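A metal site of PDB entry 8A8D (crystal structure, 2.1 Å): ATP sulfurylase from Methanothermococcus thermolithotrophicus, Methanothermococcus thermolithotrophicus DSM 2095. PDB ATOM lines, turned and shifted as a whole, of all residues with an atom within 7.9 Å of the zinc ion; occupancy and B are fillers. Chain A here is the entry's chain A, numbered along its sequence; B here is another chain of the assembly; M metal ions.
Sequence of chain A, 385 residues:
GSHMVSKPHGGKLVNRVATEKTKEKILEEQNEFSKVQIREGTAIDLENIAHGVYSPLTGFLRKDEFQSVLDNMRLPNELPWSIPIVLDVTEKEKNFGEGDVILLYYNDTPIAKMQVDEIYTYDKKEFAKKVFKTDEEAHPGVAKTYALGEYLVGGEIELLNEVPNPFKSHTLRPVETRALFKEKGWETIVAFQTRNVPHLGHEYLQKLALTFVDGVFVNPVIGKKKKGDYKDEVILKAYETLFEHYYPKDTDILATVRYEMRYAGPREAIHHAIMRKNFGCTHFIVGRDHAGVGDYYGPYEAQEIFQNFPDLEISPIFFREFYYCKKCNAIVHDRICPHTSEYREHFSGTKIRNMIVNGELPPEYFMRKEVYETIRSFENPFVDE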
ATOM      1  N   TYR A 323       3.155  18.985 -28.295  1.00  0.00           N
ATOM      2  CA  TYR A 323       4.306  18.164 -27.916  1.00  0.00           C
ATOM      3  C   TYR A 323       3.786  16.949 -27.169  1.00  0.00           C
ATOM      4  O   TYR A 323       2.650  16.923 -26.688  1.00  0.00           O
ATOM      5  CB  TYR A 323       5.275  18.950 -27.035  1.00  0.00           C
ATOM      6  CG  TYR A 323       4.628  19.574 -25.816  1.00  0.00           C
ATOM      7  CD1 TYR A 323       4.486  18.865 -24.634  1.00  0.00           C
ATOM      8  CD2 TYR A 323       4.131  20.873 -25.864  1.00  0.00           C
ATOM      9  CE1 TYR A 323       3.878  19.426 -23.533  1.00  0.00           C
ATOM     10  CE2 TYR A 323       3.526  21.448 -24.768  1.00  0.00           C
ATOM     11  CZ  TYR A 323       3.403  20.720 -23.601  1.00  0.00           C
ATOM     12  OH  TYR A 323       2.803  21.287 -22.503  1.00  0.00           O
ATOM     13  N   TYR A 324       4.635  15.935 -27.060  1.00  0.00           N
ATOM     14  CA  TYR A 324       4.320  14.772 -26.250  1.00  0.00           C
ATOM     15  C   TYR A 324       4.778  15.021 -24.820  1.00  0.00           C
ATOM     16  O   TYR A 324       5.910  15.461 -24.590  1.00  0.00           O
ATOM     17  CB  TYR A 324       4.974  13.501 -26.792  1.00  0.00           C
ATOM     18  CG  TYR A 324       4.495  12.270 -26.064  1.00  0.00           C
ATOM     19  CD1 TYR A 324       3.355  11.598 -26.472  1.00  0.00           C
ATOM     20  CD2 TYR A 324       5.172  11.792 -24.948  1.00  0.00           C
ATOM     21  CE1 TYR A 324       2.894  10.487 -25.802  1.00  0.00           C
ATOM     22  CE2 TYR A 324       4.722  10.669 -24.262  1.00  0.00           C
ATOM     23  CZ  TYR A 324       3.590  10.028 -24.705  1.00  0.00           C
ATOM     24  OH  TYR A 324       3.133   8.906 -24.041  1.00  0.00           O
ATOM     25  N   CYS A 325       3.890  14.747 -23.863  1.00  0.00           N
ATOM     26  CA  CYS A 325       4.206  14.864 -22.448  1.00  0.00           C
ATOM     27  C   CYS A 325       4.315  13.463 -21.842  1.00  0.00           C
ATOM     28  O   CYS A 325       3.404  12.648 -21.986  1.00  0.00           O
ATOM     29  CB  CYS A 325       3.138  15.663 -21.708  1.00  0.00           C
ATOM     30  SG  CYS A 325       3.445  15.823 -19.955  1.00  0.00           S
ATOM     31  N   LYS A 326       5.438  13.205 -21.172  1.00  0.00           N
ATOM     32  CA  LYS A 326       5.680  11.892 -20.588  1.00  0.00           C
ATOM     33  C   LYS A 326       4.999  11.708 -19.239  1.00  0.00           C
ATOM     34  O   LYS A 326       5.145  10.636 -18.644  1.00  0.00           O
ATOM     35  CB  LYS A 326       7.183  11.663 -20.447  1.00  0.00           C
ATOM     36  CG  LYS A 326       7.902  11.534 -21.785  1.00  0.00           C
ATOM     37  CD  LYS A 326       9.399  11.352 -21.608  1.00  0.00           C
ATOM     38  CE  LYS A 326      10.060  12.657 -21.218  1.00  0.00           C
ATOM     39  NZ  LYS A 326      11.534  12.623 -21.419  1.00  0.00           N
ATOM     40  N   LYS A 327       4.255  12.702 -18.757  1.00  0.00           N
ATOM     41  CA  LYS A 327       3.397  12.520 -17.590  1.00  0.00           C
ATOM     42  C   LYS A 327       1.933  12.427 -17.975  1.00  0.00           C
ATOM     43  O   LYS A 327       1.215  11.535 -17.511  1.00  0.00           O
ATOM     44  CB  LYS A 327       3.597  13.655 -16.579  1.00  0.00           C
ATOM     45  CG  LYS A 327       2.636  13.572 -15.391  1.00  0.00           C
ATOM     46  CD  LYS A 327       3.259  14.093 -14.107  1.00  0.00           C
ATOM     47  CE  LYS A 327       2.391  13.724 -12.912  1.00  0.00           C
ATOM     48  NZ  LYS A 327       2.770  14.462 -11.674  1.00  0.00           N
ATOM     49  N   CYS A 328       1.456  13.343 -18.821  1.00  0.00           N
ATOM     50  CA  CYS A 328       0.108  13.202 -19.367  1.00  0.00           C
ATOM     51  C   CYS A 328      -0.020  11.936 -20.203  1.00  0.00           C
ATOM     52  O   CYS A 328      -1.128  11.402 -20.345  1.00  0.00           O
ATOM     53  CB  CYS A 328      -0.257  14.429 -20.211  1.00  0.00           C
ATOM     54  SG  CYS A 328      -0.420  15.974 -19.290  1.00  0.00           S
ATOM     55  N   ASN A 329       1.093  11.450 -20.754  1.00  0.00           N
ATOM     56  CA  ASN A 329       1.096  10.260 -21.607  1.00  0.00           C
ATOM     57  C   ASN A 329       0.308  10.499 -22.892  1.00  0.00           C
ATOM     58  O   ASN A 329      -0.370   9.603 -23.395  1.00  0.00           O
ATOM     59  CB  ASN A 329       0.549   9.049 -20.860  1.00  0.00           C
ATOM     60  CG  ASN A 329       1.374   8.670 -19.652  1.00  0.00           C
ATOM     61  OD1 ASN A 329       2.610   8.755 -19.679  1.00  0.00           O
ATOM     62  ND2 ASN A 329       0.715   8.255 -18.581  1.00  0.00           N
ATOM     63  N   ALA A 330       0.406  11.711 -23.438  1.00  0.00           N
ATOM     64  CA  ALA A 330      -0.390  12.058 -24.614  1.00  0.00           C
ATOM     65  C   ALA A 330       0.208  13.273 -25.302  1.00  0.00           C
ATOM     66  O   ALA A 330       0.928  14.060 -24.685  1.00  0.00           O
ATOM     67  CB  ALA A 330      -1.848  12.328 -24.238  1.00  0.00           C
ATOM     68  N   VAL A 332      -0.121  16.797 -26.214  1.00  0.00           N
ATOM     69  CA  VAL A 332      -0.822  17.877 -25.531  1.00  0.00           C
ATOM     70  C   VAL A 332      -0.276  19.204 -26.043  1.00  0.00           C
ATOM     71  O   VAL A 332       0.575  19.257 -26.934  1.00  0.00           O
ATOM     72  CB  VAL A 332      -0.670  17.790 -23.995  1.00  0.00           C
ATOM     73  CG1 VAL A 332      -1.288  16.502 -23.482  1.00  0.00           C
ATOM     74  CG2 VAL A 332       0.805  17.867 -23.605  1.00  0.00           C
ATOM     75  N   HIS A 333      -0.791  20.302 -25.476  1.00  0.00           N
ATOM     76  CA  HIS A 333      -0.260  21.639 -25.734  1.00  0.00           C
ATOM     77  C   HIS A 333      -0.239  22.404 -24.419  1.00  0.00           C
ATOM     78  O   HIS A 333      -0.903  22.028 -23.449  1.00  0.00           O
ATOM     79  CB  HIS A 333      -1.081  22.376 -26.800  1.00  0.00           C
ATOM     80  CG  HIS A 333      -2.557  22.290 -26.608  1.00  0.00           C
ATOM     81  ND1 HIS A 333      -3.305  23.341 -26.104  1.00  0.00           N
ATOM     82  CD2 HIS A 333      -3.433  21.288 -26.853  1.00  0.00           C
ATOM     83  CE1 HIS A 333      -4.576  22.975 -26.042  1.00  0.00           C
ATOM     84  NE2 HIS A 333      -4.680  21.744 -26.486  1.00  0.00           N
ATOM     85  N   ILE A 336      -3.160  23.026 -21.786  1.00  0.00           N
ATOM     86  CA  ILE A 336      -3.791  21.981 -20.980  1.00  0.00           C
ATOM     87  C   ILE A 336      -2.783  21.154 -20.202  1.00  0.00           C
ATOM     88  O   ILE A 336      -3.188  20.181 -19.545  1.00  0.00           O
ATOM     89  CB  ILE A 336      -4.664  21.061 -21.858  1.00  0.00           C
ATOM     90  CG1 ILE A 336      -3.826  20.389 -22.942  1.00  0.00           C
ATOM     91  CG2 ILE A 336      -5.802  21.857 -22.487  1.00  0.00           C
ATOM     92  CD1 ILE A 336      -4.561  19.301 -23.700  1.00  0.00           C
ATOM     93  N   CYS A 337      -1.498  21.483 -20.250  1.00  0.00           N
ATOM     94  CA  CYS A 337      -0.453  20.688 -19.605  1.00  0.00           C
ATOM     95  C   CYS A 337       0.378  21.578 -18.691  1.00  0.00           C
ATOM     96  O   CYS A 337       0.966  22.577 -19.166  1.00  0.00           O
ATOM     97  CB  CYS A 337       0.426  20.009 -20.647  1.00  0.00           C
ATOM     98  SG  CYS A 337       1.913  19.267 -19.954  1.00  0.00           S
ATOM     99  N   PRO A 338       0.481  21.271 -17.400  1.00  0.00           N
ATOM    100  CA  PRO A 338       1.286  22.105 -16.484  1.00  0.00           C
ATOM    101  C   PRO A 338       2.717  21.628 -16.244  1.00  0.00           C
ATOM    102  O   PRO A 338       3.399  22.238 -15.428  1.00  0.00           O
ATOM    103  CB  PRO A 338       0.470  21.997 -15.188  1.00  0.00           C
ATOM    104  CG  PRO A 338      -0.070  20.597 -15.207  1.00  0.00           C
ATOM    105  CD  PRO A 338      -0.265  20.220 -16.669  1.00  0.00           C
ATOM    106  N   HIS A 339       3.064  20.514 -16.880  1.00  0.00           N
ATOM    107  CA  HIS A 339       4.349  19.780 -16.681  1.00  0.00           C
ATOM    108  C   HIS A 339       5.578  20.555 -17.176  1.00  0.00           C
ATOM    109  O   HIS A 339       5.467  21.270 -18.184  1.00  0.00           O
ATOM    110  CB  HIS A 339       4.177  18.345 -17.204  1.00  0.00           C
ATOM    111  CG  HIS A 339       3.044  17.662 -16.525  1.00  0.00           C
ATOM    112  ND1 HIS A 339       1.922  17.206 -17.200  1.00  0.00           N
ATOM    113  CD2 HIS A 339       2.827  17.414 -15.214  1.00  0.00           C
ATOM    114  CE1 HIS A 339       1.086  16.684 -16.334  1.00  0.00           C
ATOM    115  NE2 HIS A 339       1.613  16.797 -15.113  1.00  0.00           N
ATOM    116  N   THR A 340       6.712  20.314 -16.514  1.00  0.00           N
ATOM    117  CA  THR A 340       8.027  20.960 -16.782  1.00  0.00           C
ATOM    118  C   THR A 340       8.700  20.391 -18.045  1.00  0.00           C
ATOM    119  O   THR A 340       8.209  19.383 -18.593  1.00  0.00           O
ATOM    120  CB  THR A 340       8.895  21.013 -15.517  1.00  0.00           C
ATOM    121  OG1 THR A 340       8.899  19.736 -14.888  1.00  0.00           O
ATOM    122  CG2 THR A 340       8.429  22.056 -14.535  1.00  0.00           C
ATOM    123  N   TYR A 343       9.527  16.507 -18.916  1.00  0.00           N
ATOM    124  CA  TYR A 343       8.361  15.699 -19.367  1.00  0.00           C
ATOM    125  C   TYR A 343       8.009  15.944 -20.844  1.00  0.00           C
ATOM    126  O   TYR A 343       7.386  15.064 -21.453  1.00  0.00           O
ATOM    127  CB  TYR A 343       7.171  15.903 -18.435  1.00  0.00           C
ATOM    128  CG  TYR A 343       7.441  15.534 -17.002  1.00  0.00           C
ATOM    129  CD1 TYR A 343       7.480  14.205 -16.602  1.00  0.00           C
ATOM    130  CD2 TYR A 343       7.688  16.504 -16.049  1.00  0.00           C
ATOM    131  CE1 TYR A 343       7.739  13.851 -15.292  1.00  0.00           C
ATOM    132  CE2 TYR A 343       7.951  16.166 -14.734  1.00  0.00           C
ATOM    133  CZ  TYR A 343       7.975  14.833 -14.353  1.00  0.00           C
ATOM    134  OH  TYR A 343       8.240  14.505 -13.053  1.00  0.00           O
ATOM    135  N   ARG A 344       8.359  17.119 -21.392  1.00  0.00           N
ATOM    136  CA  ARG A 344       7.951  17.483 -22.772  1.00  0.00           C
ATOM    137  C   ARG A 344       8.922  16.972 -23.851  1.00  0.00           C
ATOM    138  O   ARG A 344      10.127  17.234 -23.740  1.00  0.00           O
ATOM    139  CB  ARG A 344       7.765  18.997 -22.879  1.00  0.00           C
ATOM    140  CG  ARG A 344       6.818  19.587 -21.843  1.00  0.00           C
ATOM    141  CD  ARG A 344       6.531  21.056 -22.055  1.00  0.00           C
ATOM    142  NE  ARG A 344       5.572  21.551 -21.088  1.00  0.00           N
ATOM    143  CZ  ARG A 344       4.875  22.671 -21.204  1.00  0.00           C
ATOM    144  NH1 ARG A 344       5.027  23.440 -22.271  1.00  0.00           N
ATOM    145  NH2 ARG A 344       4.030  23.013 -20.251  1.00  0.00           N
ATOM    146  N   GLU B 203     -11.306  13.820 -17.716  1.00  0.00           N
ATOM    147  CA  GLU B 203     -10.231  14.781 -17.940  1.00  0.00           C
ATOM    148  C   GLU B 203     -10.155  15.182 -19.408  1.00  0.00           C
ATOM    149  O   GLU B 203      -9.958  16.364 -19.724  1.00  0.00           O
ATOM    150  CB  GLU B 203      -8.901  14.178 -17.484  1.00  0.00           C
ATOM    151  CG  GLU B 203      -7.714  15.132 -17.551  1.00  0.00           C
ATOM    152  CD  GLU B 203      -6.424  14.468 -17.112  1.00  0.00           C
ATOM    153  OE1 GLU B 203      -6.507  13.367 -16.534  1.00  0.00           O
ATOM    154  OE2 GLU B 203      -5.341  15.033 -17.355  1.00  0.00           O
ATOM    155  N   LYS B 207     -10.542  19.157 -20.521  1.00  0.00           N
ATOM    156  CA  LYS B 207      -9.444  19.847 -21.179  1.00  0.00           C
ATOM    157  C   LYS B 207      -9.786  20.214 -22.618  1.00  0.00           C
ATOM    158  O   LYS B 207      -9.322  21.241 -23.127  1.00  0.00           O
ATOM    159  CB  LYS B 207      -8.182  18.987 -21.113  1.00  0.00           C
ATOM    160  CG  LYS B 207      -7.519  19.030 -19.746  1.00  0.00           C
ATOM    161  CD  LYS B 207      -6.298  18.148 -19.658  1.00  0.00           C
ATOM    162  CE  LYS B 207      -5.639  18.277 -18.291  1.00  0.00           C
ATOM    163  NZ  LYS B 207      -4.521  17.317 -18.102  1.00  0.00           N
ATOM    164  N   HIS B 245      -1.830  17.628 -10.037  1.00  0.00           N
ATOM    165  CA  HIS B 245      -0.823  16.889 -10.774  1.00  0.00           C
ATOM    166  C   HIS B 245      -0.962  17.005 -12.290  1.00  0.00           C
ATOM    167  O   HIS B 245      -0.005  16.695 -13.006  1.00  0.00           O
ATOM    168  CB  HIS B 245      -0.865  15.406 -10.395  1.00  0.00           C
ATOM    169  CG  HIS B 245      -0.178  15.098  -9.098  1.00  0.00           C
ATOM    170  ND1 HIS B 245       1.141  14.699  -9.031  1.00  0.00           N
ATOM    171  CD2 HIS B 245      -0.629  15.117  -7.821  1.00  0.00           C
ATOM    172  CE1 HIS B 245       1.469  14.507  -7.766  1.00  0.00           C
ATOM    173  NE2 HIS B 245       0.419  14.748  -7.018  1.00  0.00           N
ATOM    174  N   TYR B 246      -2.125  17.430 -12.796  1.00  0.00           N
ATOM    175  CA  TYR B 246      -2.370  17.382 -14.232  1.00  0.00           C
ATOM    176  C   TYR B 246      -3.017  18.619 -14.826  1.00  0.00           C
ATOM    177  O   TYR B 246      -3.124  18.691 -16.048  1.00  0.00           O
ATOM    178  CB  TYR B 246      -3.226  16.149 -14.562  1.00  0.00           C
ATOM    179  CG  TYR B 246      -2.501  14.848 -14.324  1.00  0.00           C
ATOM    180  CD1 TYR B 246      -2.515  14.241 -13.071  1.00  0.00           C
ATOM    181  CD2 TYR B 246      -1.784  14.230 -15.335  1.00  0.00           C
ATOM    182  CE1 TYR B 246      -1.849  13.046 -12.849  1.00  0.00           C
ATOM    183  CE2 TYR B 246      -1.115  13.044 -15.128  1.00  0.00           C
ATOM    184  CZ  TYR B 246      -1.145  12.464 -13.873  1.00  0.00           C
ATOM    185  OH  TYR B 246      -0.476  11.279 -13.666  1.00  0.00           O
ATOM    186  N   TYR B 247      -3.445  19.591 -14.023  1.00  0.00           N
ATOM    187  CA  TYR B 247      -4.111  20.769 -14.560  1.00  0.00           C
ATOM    188  C   TYR B 247      -3.271  22.023 -14.323  1.00  0.00           C
ATOM    189  O   TYR B 247      -2.670  22.174 -13.261  1.00  0.00           O
ATOM    190  CB  TYR B 247      -5.484  20.973 -13.916  1.00  0.00           C
ATOM    191  CG  TYR B 247      -6.556  20.052 -14.449  1.00  0.00           C
ATOM    192  CD1 TYR B 247      -6.401  18.672 -14.412  1.00  0.00           C
ATOM    193  CD2 TYR B 247      -7.732  20.560 -14.986  1.00  0.00           C
ATOM    194  CE1 TYR B 247      -7.372  17.824 -14.904  1.00  0.00           C
ATOM    195  CE2 TYR B 247      -8.709  19.720 -15.480  1.00  0.00           C
ATOM    196  CZ  TYR B 247      -8.528  18.359 -15.442  1.00  0.00           C
ATOM    197  OH  TYR B 247      -9.499  17.514 -15.924  1.00  0.00           O
ATOM    198  N   ARG B 368      -5.565   8.060 -13.518  1.00  0.00           N
ATOM    199  CA  ARG B 368      -4.237   8.555 -13.203  1.00  0.00           C
ATOM    200  C   ARG B 368      -3.656   7.819 -12.004  1.00  0.00           C
ATOM    201  O   ARG B 368      -4.371   7.472 -11.063  1.00  0.00           O
ATOM    202  CB  ARG B 368      -4.279  10.054 -12.939  1.00  0.00           C
ATOM    203  CG  ARG B 368      -4.759  10.896 -14.111  1.00  0.00           C
ATOM    204  CD  ARG B 368      -3.862  10.732 -15.329  1.00  0.00           C
ATOM    205  NE  ARG B 368      -4.073  11.781 -16.308  1.00  0.00           N
ATOM    206  CZ  ARG B 368      -3.430  11.860 -17.474  1.00  0.00           C
ATOM    207  NH1 ARG B 368      -2.549  10.940 -17.833  1.00  0.00           N
ATOM    208  NH2 ARG B 368      -3.684  12.881 -18.290  1.00  0.00           N
HETATM  209 ZN    ZN M   1       1.620  17.125 -19.220  1.00  0.00          ZN
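Four residues have an atom within 4 Å of the zinc ion: Cys 325, Cys 328, Cys 337 and His 339.
The backbone carbonyl oxygen (O) of Cys 337 is in hydrogen-bond range of the guanidinium group (NH2) of Arg 344. The backbone carbonyl oxygen (O) of Cys 328 is in hydrogen-bond range of the guanidinium group (NH1) of Arg 368 of chain B (2.9 Å). The backbone NH (N) of Cys 325 is in hydrogen-bond range of the backbone carbonyl oxygen (O) of Ala 330. SG of Cys 337 lies close to OH of Tyr 323. The guanidinium group of Arg 344 lies within hydrogen-bond range of the backbone carbonyl oxygen of His 339. The side-chain sulfur (SG) of Cys 325 lies close to the backbone NH (N) of Lys 327, 3.4 Å away. A ring nitrogen (NE2) of His 339 is in hydrogen-bond range of the backbone carbonyl oxygen of His 245 of chain B (2.7 Å).
The zinc ion is bound by a ring nitrogen (ND1) of His 339, at 2.0 Å. The zinc ion is bound by the side-chain sulfur (SG) of Cys 337. SG of Cys 328 is bound to the zinc ion (2.3 Å). SG of Cys 325 binds the zinc ion, at 2.4 Å. The zinc ion has four donor atoms within binding distance.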
